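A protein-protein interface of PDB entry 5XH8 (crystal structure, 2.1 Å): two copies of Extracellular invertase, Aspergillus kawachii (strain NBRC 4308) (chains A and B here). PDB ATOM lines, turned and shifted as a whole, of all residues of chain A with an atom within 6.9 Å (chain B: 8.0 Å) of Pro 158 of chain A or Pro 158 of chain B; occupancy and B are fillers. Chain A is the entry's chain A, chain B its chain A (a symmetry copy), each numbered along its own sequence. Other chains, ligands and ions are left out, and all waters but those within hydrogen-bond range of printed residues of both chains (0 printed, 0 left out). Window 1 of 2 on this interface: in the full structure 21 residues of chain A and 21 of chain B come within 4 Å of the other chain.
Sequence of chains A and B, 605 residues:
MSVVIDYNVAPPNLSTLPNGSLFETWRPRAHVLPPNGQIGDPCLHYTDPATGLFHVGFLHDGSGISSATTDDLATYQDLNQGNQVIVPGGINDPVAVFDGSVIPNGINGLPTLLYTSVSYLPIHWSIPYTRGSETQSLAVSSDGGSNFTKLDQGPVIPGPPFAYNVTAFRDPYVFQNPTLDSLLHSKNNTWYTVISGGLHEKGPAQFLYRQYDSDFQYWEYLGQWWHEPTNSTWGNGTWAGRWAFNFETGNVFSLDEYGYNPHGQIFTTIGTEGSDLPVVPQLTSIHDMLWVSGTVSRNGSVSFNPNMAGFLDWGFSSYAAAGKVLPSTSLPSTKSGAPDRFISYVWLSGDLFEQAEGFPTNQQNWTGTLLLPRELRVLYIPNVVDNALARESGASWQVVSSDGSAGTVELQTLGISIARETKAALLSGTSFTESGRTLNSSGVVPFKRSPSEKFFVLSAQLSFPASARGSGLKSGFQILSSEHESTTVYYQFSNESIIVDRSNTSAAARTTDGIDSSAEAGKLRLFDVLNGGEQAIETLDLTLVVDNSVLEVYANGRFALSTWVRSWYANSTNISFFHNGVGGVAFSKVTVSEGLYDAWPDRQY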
ATOM      1  N   ARG A 131     -15.808   3.656  -5.762  1.00  0.00           N
ATOM      2  CA  ARG A 131     -15.223   4.543  -4.763  1.00  0.00           C
ATOM      3  C   ARG A 131     -13.929   5.181  -5.277  1.00  0.00           C
ATOM      4  O   ARG A 131     -13.080   4.503  -5.845  1.00  0.00           O
ATOM      5  CB  ARG A 131     -14.937   3.742  -3.472  1.00  0.00           C
ATOM      6  CG  ARG A 131     -14.364   4.554  -2.302  1.00  0.00           C
ATOM      7  CD  ARG A 131     -15.443   5.284  -1.560  1.00  0.00           C
ATOM      8  NE  ARG A 131     -14.906   6.006  -0.419  1.00  0.00           N
ATOM      9  CZ  ARG A 131     -14.610   5.462   0.758  1.00  0.00           C
ATOM     10  NH1 ARG A 131     -14.750   4.155   0.981  1.00  0.00           N
ATOM     11  NH2 ARG A 131     -14.131   6.231   1.720  1.00  0.00           N
ATOM     12  N   GLY A 132     -13.790   6.491  -5.093  1.00  0.00           N
ATOM     13  CA  GLY A 132     -12.589   7.186  -5.537  1.00  0.00           C
ATOM     14  C   GLY A 132     -12.448   7.365  -7.046  1.00  0.00           C
ATOM     15  O   GLY A 132     -11.405   7.816  -7.500  1.00  0.00           O
ATOM     16  N   SER A 133     -13.474   7.048  -7.845  1.00  0.00           N
ATOM     17  CA  SER A 133     -13.350   7.252  -9.292  1.00  0.00           C
ATOM     18  C   SER A 133     -13.148   8.759  -9.679  1.00  0.00           C
ATOM     19  O   SER A 133     -12.401   9.060 -10.617  1.00  0.00           O
ATOM     20  CB  SER A 133     -14.484   6.552 -10.070  1.00  0.00           C
ATOM     21  OG  SER A 133     -15.725   6.994  -9.652  1.00  0.00           O
ATOM     22  N   GLU A 134     -13.746   9.673  -8.910  1.00  0.00           N
ATOM     23  CA  GLU A 134     -13.678  11.097  -9.154  1.00  0.00           C
ATOM     24  C   GLU A 134     -13.208  11.850  -7.890  1.00  0.00           C
ATOM     25  O   GLU A 134     -13.859  11.800  -6.831  1.00  0.00           O
ATOM     26  CB  GLU A 134     -15.039  11.617  -9.613  1.00  0.00           C
ATOM     27  CG  GLU A 134     -15.580  10.942 -10.878  1.00  0.00           C
ATOM     28  CD  GLU A 134     -17.034  11.262 -11.122  1.00  0.00           C
ATOM     29  OE1 GLU A 134     -17.832  11.116 -10.155  1.00  0.00           O
ATOM     30  OE2 GLU A 134     -17.372  11.673 -12.263  1.00  0.00           O
ATOM     31  N   THR A 135     -12.067  12.517  -8.007  1.00  0.00           N
ATOM     32  CA  THR A 135     -11.550  13.393  -6.962  1.00  0.00           C
ATOM     33  C   THR A 135     -11.412  14.785  -7.566  1.00  0.00           C
ATOM     34  O   THR A 135     -11.532  14.965  -8.786  1.00  0.00           O
ATOM     35  CB  THR A 135     -10.209  12.897  -6.420  1.00  0.00           C
ATOM     36  OG1 THR A 135      -9.247  12.825  -7.473  1.00  0.00           O
ATOM     37  CG2 THR A 135     -10.342  11.501  -5.810  1.00  0.00           C
ATOM     38  N   GLN A 136     -11.207  15.783  -6.719  1.00  0.00           N
ATOM     39  CA  GLN A 136     -11.003  17.148  -7.212  1.00  0.00           C
ATOM     40  C   GLN A 136      -9.591  17.588  -6.837  1.00  0.00           C
ATOM     41  O   GLN A 136      -9.213  17.533  -5.646  1.00  0.00           O
ATOM     42  CB  GLN A 136     -12.069  18.118  -6.688  1.00  0.00           C
ATOM     43  CG  GLN A 136     -13.448  17.500  -6.454  1.00  0.00           C
ATOM     44  CD  GLN A 136     -14.046  16.886  -7.701  1.00  0.00           C
ATOM     45  OE1 GLN A 136     -13.860  17.384  -8.817  1.00  0.00           O
ATOM     46  NE2 GLN A 136     -14.789  15.799  -7.516  1.00  0.00           N
ATOM     47  N   GLY A 154      -1.855  15.150  -3.449  1.00  0.00           N
ATOM     48  CA  GLY A 154      -3.128  14.493  -3.663  1.00  0.00           C
ATOM     49  C   GLY A 154      -4.269  15.463  -3.901  1.00  0.00           C
ATOM     50  O   GLY A 154      -4.091  16.687  -3.797  1.00  0.00           O
ATOM     51  N   PRO A 155      -5.456  14.919  -4.234  1.00  0.00           N
ATOM     52  CA  PRO A 155      -6.640  15.745  -4.412  1.00  0.00           C
ATOM     53  C   PRO A 155      -6.974  16.569  -3.148  1.00  0.00           C
ATOM     54  O   PRO A 155      -6.767  16.113  -2.008  1.00  0.00           O
ATOM     55  CB  PRO A 155      -7.754  14.736  -4.683  1.00  0.00           C
ATOM     56  CG  PRO A 155      -7.240  13.420  -4.167  1.00  0.00           C
ATOM     57  CD  PRO A 155      -5.749  13.476  -4.322  1.00  0.00           C
ATOM     58  N   VAL A 156      -7.481  17.771  -3.371  1.00  0.00           N
ATOM     59  CA  VAL A 156      -7.918  18.639  -2.270  1.00  0.00           C
ATOM     60  C   VAL A 156      -9.324  18.258  -1.796  1.00  0.00           C
ATOM     61  O   VAL A 156      -9.704  18.559  -0.651  1.00  0.00           O
ATOM     62  CB  VAL A 156      -7.807  20.135  -2.625  1.00  0.00           C
ATOM     63  CG1 VAL A 156      -6.355  20.496  -2.893  1.00  0.00           C
ATOM     64  CG2 VAL A 156      -8.654  20.518  -3.815  1.00  0.00           C
ATOM     65  N   ILE A 157     -10.078  17.579  -2.656  1.00  0.00           N
ATOM     66  CA  ILE A 157     -11.357  16.977  -2.262  1.00  0.00           C
ATOM     67  C   ILE A 157     -11.320  15.512  -2.715  1.00  0.00           C
ATOM     68  O   ILE A 157     -11.660  15.231  -3.877  1.00  0.00           O
ATOM     69  CB  ILE A 157     -12.584  17.732  -2.830  1.00  0.00           C
ATOM     70  CG1 ILE A 157     -12.571  19.198  -2.405  1.00  0.00           C
ATOM     71  CG2 ILE A 157     -13.872  17.046  -2.394  1.00  0.00           C
ATOM     72  CD1 ILE A 157     -13.642  20.055  -3.052  1.00  0.00           C
ATOM     73  N   PRO A 158     -10.896  14.586  -1.810  1.00  0.00           N
ATOM     74  CA  PRO A 158     -10.695  13.158  -2.171  1.00  0.00           C
ATOM     75  C   PRO A 158     -11.933  12.303  -2.377  1.00  0.00           C
ATOM     76  O   PRO A 158     -11.837  11.150  -2.806  1.00  0.00           O
ATOM     77  CB  PRO A 158      -9.889  12.580  -0.984  1.00  0.00           C
ATOM     78  CG  PRO A 158      -9.468  13.721  -0.141  1.00  0.00           C
ATOM     79  CD  PRO A 158     -10.353  14.893  -0.466  1.00  0.00           C
ATOM     80  N   GLY A 159     -13.092  12.824  -2.067  1.00  0.00           N
ATOM     81  CA  GLY A 159     -14.303  12.098  -2.363  1.00  0.00           C
ATOM     82  C   GLY A 159     -15.448  12.858  -1.773  1.00  0.00           C
ATOM     83  O   GLY A 159     -15.239  13.941  -1.193  1.00  0.00           O
ATOM     84  N   PRO A 160     -16.659  12.308  -1.929  1.00  0.00           N
ATOM     85  CA  PRO A 160     -17.850  12.964  -1.432  1.00  0.00           C
ATOM     86  C   PRO A 160     -17.967  12.839   0.085  1.00  0.00           C
ATOM     87  O   PRO A 160     -17.185  12.128   0.690  1.00  0.00           O
ATOM     88  CB  PRO A 160     -18.978  12.222  -2.141  1.00  0.00           C
ATOM     89  CG  PRO A 160     -18.441  10.888  -2.447  1.00  0.00           C
ATOM     90  CD  PRO A 160     -16.963  11.045  -2.624  1.00  0.00           C
ATOM     91  N   PHE A 169     -19.894  12.744  -9.100  1.00  0.00           N
ATOM     92  CA  PHE A 169     -19.275  13.721  -8.220  1.00  0.00           C
ATOM     93  C   PHE A 169     -18.162  14.483  -8.954  1.00  0.00           C
ATOM     94  O   PHE A 169     -16.973  14.208  -8.774  1.00  0.00           O
ATOM     95  CB  PHE A 169     -18.754  13.005  -6.977  1.00  0.00           C
ATOM     96  CG  PHE A 169     -18.320  13.927  -5.880  1.00  0.00           C
ATOM     97  CD1 PHE A 169     -19.250  14.646  -5.158  1.00  0.00           C
ATOM     98  CD2 PHE A 169     -16.996  14.030  -5.539  1.00  0.00           C
ATOM     99  CE1 PHE A 169     -18.851  15.503  -4.148  1.00  0.00           C
ATOM    100  CE2 PHE A 169     -16.587  14.873  -4.518  1.00  0.00           C
ATOM    101  CZ  PHE A 169     -17.523  15.606  -3.814  1.00  0.00           C
ATOM    102  N   SER B 117      -1.374   2.775   1.421  1.00  0.00           N
ATOM    103  CA  SER B 117      -1.041   2.958   0.016  1.00  0.00           C
ATOM    104  C   SER B 117      -0.396   4.352  -0.155  1.00  0.00           C
ATOM    105  O   SER B 117      -0.992   5.351   0.228  1.00  0.00           O
ATOM    106  CB  SER B 117      -2.306   2.793  -0.828  1.00  0.00           C
ATOM    107  OG  SER B 117      -3.444   3.405  -0.241  1.00  0.00           O
ATOM    108  N   TYR B 129       3.882  17.972   5.644  1.00  0.00           N
ATOM    109  CA  TYR B 129       3.222  16.797   5.109  1.00  0.00           C
ATOM    110  C   TYR B 129       2.626  17.076   3.719  1.00  0.00           C
ATOM    111  O   TYR B 129       1.940  18.084   3.522  1.00  0.00           O
ATOM    112  CB  TYR B 129       2.124  16.388   6.076  1.00  0.00           C
ATOM    113  CG  TYR B 129       1.570  15.024   5.843  1.00  0.00           C
ATOM    114  CD1 TYR B 129       2.214  13.898   6.352  1.00  0.00           C
ATOM    115  CD2 TYR B 129       0.428  14.845   5.073  1.00  0.00           C
ATOM    116  CE1 TYR B 129       1.707  12.625   6.138  1.00  0.00           C
ATOM    117  CE2 TYR B 129      -0.088  13.583   4.853  1.00  0.00           C
ATOM    118  CZ  TYR B 129       0.549  12.473   5.384  1.00  0.00           C
ATOM    119  OH  TYR B 129       0.011  11.217   5.184  1.00  0.00           O
ATOM    120  N   ARG B 131      -0.178  16.471   1.215  1.00  0.00           N
ATOM    121  CA  ARG B 131      -1.567  16.027   1.203  1.00  0.00           C
ATOM    122  C   ARG B 131      -1.742  14.772   0.343  1.00  0.00           C
ATOM    123  O   ARG B 131      -1.224  14.696  -0.766  1.00  0.00           O
ATOM    124  CB  ARG B 131      -2.463  17.165   0.659  1.00  0.00           C
ATOM    125  CG  ARG B 131      -3.968  16.867   0.633  1.00  0.00           C
ATOM    126  CD  ARG B 131      -4.592  17.077   1.981  1.00  0.00           C
ATOM    127  NE  ARG B 131      -6.027  16.850   1.941  1.00  0.00           N
ATOM    128  CZ  ARG B 131      -6.926  17.727   1.505  1.00  0.00           C
ATOM    129  NH1 ARG B 131      -6.567  18.914   1.013  1.00  0.00           N
ATOM    130  NH2 ARG B 131      -8.206  17.400   1.525  1.00  0.00           N
ATOM    131  N   GLY B 132      -2.457  13.780   0.866  1.00  0.00           N
ATOM    132  CA  GLY B 132      -2.688  12.549   0.121  1.00  0.00           C
ATOM    133  C   GLY B 132      -1.482  11.627  -0.024  1.00  0.00           C
ATOM    134  O   GLY B 132      -1.563  10.645  -0.749  1.00  0.00           O
ATOM    135  N   SER B 133      -0.363  11.893   0.662  1.00  0.00           N
ATOM    136  CA  SER B 133       0.785  10.987   0.549  1.00  0.00           C
ATOM    137  C   SER B 133       0.472   9.542   1.071  1.00  0.00           C
ATOM    138  O   SER B 133       0.958   8.560   0.497  1.00  0.00           O
ATOM    139  CB  SER B 133       2.066  11.606   1.146  1.00  0.00           C
ATOM    140  OG  SER B 133       1.885  11.949   2.473  1.00  0.00           O
ATOM    141  N   GLU B 134      -0.386   9.431   2.088  1.00  0.00           N
ATOM    142  CA  GLU B 134      -0.752   8.171   2.698  1.00  0.00           C
ATOM    143  C   GLU B 134      -2.287   8.006   2.741  1.00  0.00           C
ATOM    144  O   GLU B 134      -3.005   8.811   3.361  1.00  0.00           O
ATOM    145  CB  GLU B 134      -0.163   8.077   4.104  1.00  0.00           C
ATOM    146  CG  GLU B 134       1.362   8.209   4.161  1.00  0.00           C
ATOM    147  CD  GLU B 134       1.869   8.411   5.568  1.00  0.00           C
ATOM    148  OE1 GLU B 134       1.311   9.305   6.264  1.00  0.00           O
ATOM    149  OE2 GLU B 134       2.802   7.673   5.980  1.00  0.00           O
ATOM    150  N   THR B 135      -2.776   6.978   2.057  1.00  0.00           N
ATOM    151  CA  THR B 135      -4.181   6.593   2.103  1.00  0.00           C
ATOM    152  C   THR B 135      -4.240   5.158   2.609  1.00  0.00           C
ATOM    153  O   THR B 135      -3.211   4.475   2.714  1.00  0.00           O
ATOM    154  CB  THR B 135      -4.846   6.716   0.731  1.00  0.00           C
ATOM    155  OG1 THR B 135      -4.176   5.887  -0.218  1.00  0.00           O
ATOM    156  CG2 THR B 135      -4.792   8.156   0.218  1.00  0.00           C
ATOM    157  N   GLN B 136      -5.431   4.704   2.972  1.00  0.00           N
ATOM    158  CA  GLN B 136      -5.596   3.317   3.417  1.00  0.00           C
ATOM    159  C   GLN B 136      -6.502   2.598   2.422  1.00  0.00           C
ATOM    160  O   GLN B 136      -7.630   3.067   2.151  1.00  0.00           O
ATOM    161  CB  GLN B 136      -6.127   3.228   4.852  1.00  0.00           C
ATOM    162  CG  GLN B 136      -5.692   4.366   5.775  1.00  0.00           C
ATOM    163  CD  GLN B 136      -4.189   4.482   5.913  1.00  0.00           C
ATOM    164  OE1 GLN B 136      -3.463   3.481   5.911  1.00  0.00           O
ATOM    165  NE2 GLN B 136      -3.710   5.714   6.051  1.00  0.00           N
ATOM    166  N   SER B 137      -6.001   1.479   1.882  1.00  0.00           N
ATOM    167  CA  SER B 137      -6.635   0.736   0.799  1.00  0.00           C
ATOM    168  C   SER B 137      -6.848  -0.699   1.195  1.00  0.00           C
ATOM    169  O   SER B 137      -6.219  -1.191   2.153  1.00  0.00           O
ATOM    170  CB  SER B 137      -5.783   0.812  -0.474  1.00  0.00           C
ATOM    171  OG  SER B 137      -5.775   2.138  -0.988  1.00  0.00           O
ATOM    172  N   GLY B 154     -10.733   3.102  -5.267  1.00  0.00           N
ATOM    173  CA  GLY B 154      -9.922   4.013  -4.487  1.00  0.00           C
ATOM    174  C   GLY B 154      -9.766   3.587  -3.039  1.00  0.00           C
ATOM    175  O   GLY B 154     -10.389   2.609  -2.598  1.00  0.00           O
ATOM    176  N   PRO B 155      -8.919   4.319  -2.289  1.00  0.00           N
ATOM    177  CA  PRO B 155      -8.747   4.051  -0.870  1.00  0.00           C
ATOM    178  C   PRO B 155     -10.079   4.146  -0.091  1.00  0.00           C
ATOM    179  O   PRO B 155     -10.954   4.971  -0.410  1.00  0.00           O
ATOM    180  CB  PRO B 155      -7.793   5.148  -0.403  1.00  0.00           C
ATOM    181  CG  PRO B 155      -7.875   6.226  -1.449  1.00  0.00           C
ATOM    182  CD  PRO B 155      -8.191   5.522  -2.734  1.00  0.00           C
ATOM    183  N   VAL B 156     -10.210   3.296   0.915  1.00  0.00           N
ATOM    184  CA  VAL B 156     -11.386   3.319   1.794  1.00  0.00           C
ATOM    185  C   VAL B 156     -11.245   4.398   2.872  1.00  0.00           C
ATOM    186  O   VAL B 156     -12.254   4.863   3.431  1.00  0.00           O
ATOM    187  CB  VAL B 156     -11.695   1.932   2.392  1.00  0.00           C
ATOM    188  CG1 VAL B 156     -12.022   0.950   1.279  1.00  0.00           C
ATOM    189  CG2 VAL B 156     -10.563   1.392   3.232  1.00  0.00           C
ATOM    190  N   ILE B 157     -10.010   4.811   3.142  1.00  0.00           N
ATOM    191  CA  ILE B 157      -9.749   5.975   3.996  1.00  0.00           C
ATOM    192  C   ILE B 157      -8.789   6.890   3.226  1.00  0.00           C
ATOM    193  O   ILE B 157      -7.566   6.683   3.304  1.00  0.00           O
ATOM    194  CB  ILE B 157      -9.196   5.592   5.391  1.00  0.00           C
ATOM    195  CG1 ILE B 157     -10.147   4.644   6.117  1.00  0.00           C
ATOM    196  CG2 ILE B 157      -8.937   6.845   6.217  1.00  0.00           C
ATOM    197  CD1 ILE B 157      -9.610   4.081   7.419  1.00  0.00           C
ATOM    198  N   PRO B 158      -9.337   7.885   2.474  1.00  0.00           N
ATOM    199  CA  PRO B 158      -8.519   8.751   1.585  1.00  0.00           C
ATOM    200  C   PRO B 158      -7.647   9.806   2.239  1.00  0.00           C
ATOM    201  O   PRO B 158      -6.847  10.466   1.569  1.00  0.00           O
ATOM    202  CB  PRO B 158      -9.562   9.459   0.687  1.00  0.00           C
ATOM    203  CG  PRO B 158     -10.867   8.806   0.929  1.00  0.00           C
ATOM    204  CD  PRO B 158     -10.789   8.079   2.244  1.00  0.00           C
ATOM    205  N   GLY B 159      -7.788  10.003   3.525  1.00  0.00           N
ATOM    206  CA  GLY B 159      -6.895  10.905   4.212  1.00  0.00           C
ATOM    207  C   GLY B 159      -7.380  11.044   5.619  1.00  0.00           C
ATOM    208  O   GLY B 159      -8.371  10.393   6.000  1.00  0.00           O
ATOM    209  N   PRO B 160      -6.679  11.875   6.401  1.00  0.00           N
ATOM    210  CA  PRO B 160      -7.027  12.069   7.793  1.00  0.00           C
ATOM    211  C   PRO B 160      -8.269  12.944   7.943  1.00  0.00           C
ATOM    212  O   PRO B 160      -8.743  13.485   6.961  1.00  0.00           O
ATOM    213  CB  PRO B 160      -5.791  12.751   8.369  1.00  0.00           C
ATOM    214  CG  PRO B 160      -5.155  13.438   7.236  1.00  0.00           C
ATOM    215  CD  PRO B 160      -5.487  12.649   6.008  1.00  0.00           C
ATOM    216  N   PRO B 161      -8.777  13.096   9.172  1.00  0.00           N
ATOM    217  CA  PRO B 161      -9.940  13.960   9.389  1.00  0.00           C
ATOM    218  C   PRO B 161      -9.724  15.371   8.864  1.00  0.00           C
ATOM    219  O   PRO B 161      -8.567  15.830   8.730  1.00  0.00           O
ATOM    220  CB  PRO B 161     -10.127  13.939  10.915  1.00  0.00           C
ATOM    221  CG  PRO B 161      -9.555  12.609  11.335  1.00  0.00           C
ATOM    222  CD  PRO B 161      -8.384  12.388  10.409  1.00  0.00           C
ATOM    223  N   PHE B 162     -10.836  16.003   8.503  1.00  0.00           N
ATOM    224  CA  PHE B 162     -10.847  17.268   7.775  1.00  0.00           C
ATOM    225  C   PHE B 162      -9.857  18.296   8.329  1.00  0.00           C
ATOM    226  O   PHE B 162      -9.907  18.646   9.506  1.00  0.00           O
ATOM    227  CB  PHE B 162     -12.267  17.864   7.784  1.00  0.00           C
ATOM    228  CG  PHE B 162     -12.376  19.178   7.047  1.00  0.00           C
ATOM    229  CD1 PHE B 162     -12.332  19.207   5.664  1.00  0.00           C
ATOM    230  CD2 PHE B 162     -12.478  20.385   7.744  1.00  0.00           C
ATOM    231  CE1 PHE B 162     -12.411  20.401   4.961  1.00  0.00           C
ATOM    232  CE2 PHE B 162     -12.555  21.597   7.056  1.00  0.00           C
ATOM    233  CZ  PHE B 162     -12.525  21.599   5.657  1.00  0.00           C
ATOM    234  N   PHE B 169       0.346   9.349   8.924  1.00  0.00           N
ATOM    235  CA  PHE B 169      -0.986   8.764   8.918  1.00  0.00           C
ATOM    236  C   PHE B 169      -0.965   7.377   8.260  1.00  0.00           C
ATOM    237  O   PHE B 169      -1.356   7.212   7.102  1.00  0.00           O
ATOM    238  CB  PHE B 169      -1.940   9.719   8.206  1.00  0.00           C
ATOM    239  CG  PHE B 169      -3.385   9.355   8.349  1.00  0.00           C
ATOM    240  CD1 PHE B 169      -4.030   9.505   9.560  1.00  0.00           C
ATOM    241  CD2 PHE B 169      -4.105   8.920   7.267  1.00  0.00           C
ATOM    242  CE1 PHE B 169      -5.364   9.164   9.697  1.00  0.00           C
ATOM    243  CE2 PHE B 169      -5.446   8.591   7.389  1.00  0.00           C
ATOM    244  CZ  PHE B 169      -6.079   8.723   8.610  1.00  0.00           C
ATOM    245  N   TYR B 209     -10.818   4.367  14.595  1.00  0.00           N
ATOM    246  CA  TYR B 209     -11.960   4.221  13.704  1.00  0.00           C
ATOM    247  C   TYR B 209     -12.724   2.944  13.981  1.00  0.00           C
ATOM    248  O   TYR B 209     -12.166   1.980  14.488  1.00  0.00           O
ATOM    249  CB  TYR B 209     -11.502   4.164  12.215  1.00  0.00           C
ATOM    250  CG  TYR B 209     -10.823   5.397  11.708  1.00  0.00           C
ATOM    251  CD1 TYR B 209      -9.498   5.663  12.030  1.00  0.00           C
ATOM    252  CD2 TYR B 209     -11.493   6.301  10.896  1.00  0.00           C
ATOM    253  CE1 TYR B 209      -8.871   6.806  11.574  1.00  0.00           C
ATOM    254  CE2 TYR B 209     -10.869   7.442  10.430  1.00  0.00           C
ATOM    255  CZ  TYR B 209      -9.549   7.676  10.767  1.00  0.00           C
ATOM    256  OH  TYR B 209      -8.924   8.805  10.337  1.00  0.00           O
ATOM    257  N   GLN B 217     -16.037  -0.751   3.772  1.00  0.00           N
ATOM    258  CA  GLN B 217     -15.906   0.344   2.809  1.00  0.00           C
ATOM    259  C   GLN B 217     -15.664   1.663   3.523  1.00  0.00           C
ATOM    260  O   GLN B 217     -14.818   2.467   3.111  1.00  0.00           O
ATOM    261  CB  GLN B 217     -17.176   0.397   1.962  1.00  0.00           C
ATOM    262  CG  GLN B 217     -17.132   1.296   0.751  1.00  0.00           C
ATOM    263  CD  GLN B 217     -16.061   0.895  -0.244  1.00  0.00           C
ATOM    264  OE1 GLN B 217     -15.891  -0.279  -0.559  1.00  0.00           O
ATOM    265  NE2 GLN B 217     -15.326   1.862  -0.716  1.00  0.00           N
ATOM    266  N   TYR B 218     -16.407   1.873   4.613  1.00  0.00           N
ATOM    267  CA  TYR B 218     -16.420   3.124   5.320  1.00  0.00           C
ATOM    268  C   TYR B 218     -16.025   2.912   6.765  1.00  0.00           C
ATOM    269  O   TYR B 218     -16.410   1.905   7.407  1.00  0.00           O
ATOM    270  CB  TYR B 218     -17.799   3.789   5.203  1.00  0.00           C
ATOM    271  CG  TYR B 218     -18.161   4.149   3.788  1.00  0.00           C
ATOM    272  CD1 TYR B 218     -17.514   5.209   3.146  1.00  0.00           C
ATOM    273  CD2 TYR B 218     -19.141   3.426   3.068  1.00  0.00           C
ATOM    274  CE1 TYR B 218     -17.815   5.540   1.821  1.00  0.00           C
ATOM    275  CE2 TYR B 218     -19.459   3.767   1.746  1.00  0.00           C
ATOM    276  CZ  TYR B 218     -18.779   4.833   1.131  1.00  0.00           C
ATOM    277  OH  TYR B 218     -19.036   5.214  -0.172  1.00  0.00           O
ATOM    278  N   TRP B 219     -15.244   3.865   7.261  1.00  0.00           N
ATOM    279  CA  TRP B 219     -14.646   3.793   8.583  1.00  0.00           C
ATOM    280  C   TRP B 219     -14.961   5.070   9.339  1.00  0.00           C
ATOM    281  O   TRP B 219     -14.502   6.167   8.986  1.00  0.00           O
ATOM    282  CB  TRP B 219     -13.127   3.529   8.468  1.00  0.00           C
ATOM    283  CG  TRP B 219     -12.898   2.171   7.906  1.00  0.00           C
ATOM    284  CD1 TRP B 219     -12.897   1.827   6.592  1.00  0.00           C
ATOM    285  CD2 TRP B 219     -12.711   0.957   8.645  1.00  0.00           C
ATOM    286  NE1 TRP B 219     -12.714   0.473   6.455  1.00  0.00           N
ATOM    287  CE2 TRP B 219     -12.595  -0.082   7.705  1.00  0.00           C
ATOM    288  CE3 TRP B 219     -12.657   0.648  10.014  1.00  0.00           C
ATOM    289  CZ2 TRP B 219     -12.414  -1.406   8.083  1.00  0.00           C
ATOM    290  CZ3 TRP B 219     -12.470  -0.669  10.390  1.00  0.00           C
ATOM    291  CH2 TRP B 219     -12.350  -1.680   9.437  1.00  0.00           C
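The backbone carbonyl oxygen (O) of Arg 131 of chain A is in hydrogen-bond range of the backbone NH (N) of Gly 154 of chain B (2.8 Å). The backbone carbonyl oxygen (O) of Val 156 of chain B lies within hydrogen-bond range of the guanidinium group (NH2) of Arg 131 of chain A (2.9 Å). The guanidinium group (NH1) of Arg 131 of chain A sits at hydrogen-bond distance from the backbone carbonyl oxygen (O) of Gln 217 of chain B (2.7 Å). The backbone carbonyl oxygen (O) of Arg 131 of chain B is in hydrogen-bond range of the backbone NH (N) of Gly 154 of chain A, 2.8 Å away. The backbone carbonyl oxygen (O) of Val 156 of chain A sits at hydrogen-bond distance from the guanidinium group (NH2) of Arg 131 of chain B (2.9 Å).
O of Gln 136 of chain A is in hydrogen-bond range of N of Val 156 of chain A (2.9 Å). The backbone carbonyl oxygen (O) of Gln 136 of chain B sits at hydrogen-bond distance from the backbone NH (N) of Val 156 of chain B, at 2.9 Å.
CZ of Arg 131 of chain A touches O of Pro 155 of chain B, 3.9 Å away. NH2 of Arg 131 of chain A touches CD of Pro 158 of chain B, 3.9 Å away. Arg 131 of chain A touches Tyr 218 of chain B. O of Pro 155 of chain A touches CZ of Arg 131 of chain B, 3.9 Å away. Pro 158 of chain A touches Arg 131 of chain B (CD to NH2, 3.9 Å). Pro 158 of chain A touches Pro 158 of chain B (CB to CB, 3.6 Å).
Printed residues of chain B within 4 Å of Pro 158 of chain A: Arg 131 and Pro 158. Of chain A, only Arg 131 (3.9 Å) and Pro 158 (3.6 Å) come within 4 Å of Pro 158 of chain B. No residue of chain B comes within 4 Å of Gly 159 of chain A. Printed residues of chain B within 4 Å of Gly 154 of chain A: Arg 131. Of the printed residues of chain A, Arg 131 of chain B touches Gly 154 (2.8 Å), Pro 155 (3.9 Å), Val 156 (2.9 Å) and Pro 158 (3.9 Å). Of the printed residues of chain A, Pro 155 of chain B touches Arg 131 (3.9 Å). Ser 133 of chain A touches none of the printed residues of chain B. Ile 157 of chain B touches none of the printed residues of chain A. The nearest residue of chain B that does not touch Pro 158 of chain A is Gly 159 of chain B (5.5 Å).
Of the 14 printed residues of chain A, 5 touch a printed residue of chain B. Hydrophobic or aromatic side chains of chain A that line the printed part of chain B: Pro 158. Along chain A the printed residues that touch a printed residue of chain B span positions 131 to 158. Hydrophobic or aromatic side chains of chain B that line the printed part of chain A: Pro 158 and Tyr 218. Among the printed residues, 11 pairs touch across the chains. Among the printed residues, no Asp or Glu carboxylate lies within 4 Å of a Lys or Arg side-chain nitrogen of the other chain.
Arg 131 of chain A touches Pro 155 of chain B, and with the chains exchanged Pro 155 of chain A touches Arg 131 of chain B. Arg 131 of chain A touches Pro 158 of chain B, and with the chains exchanged Pro 158 of chain A touches Arg 131 of chain B. Positions printed for both chains: 131, 132, 133, 134, 135, 136, 154, 155, 156, 157, 158, 159, 160 and 169. Of the 11 pairs that touch across the chains among the printed residues, 9 have their exchanged pair printed and touching as well.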
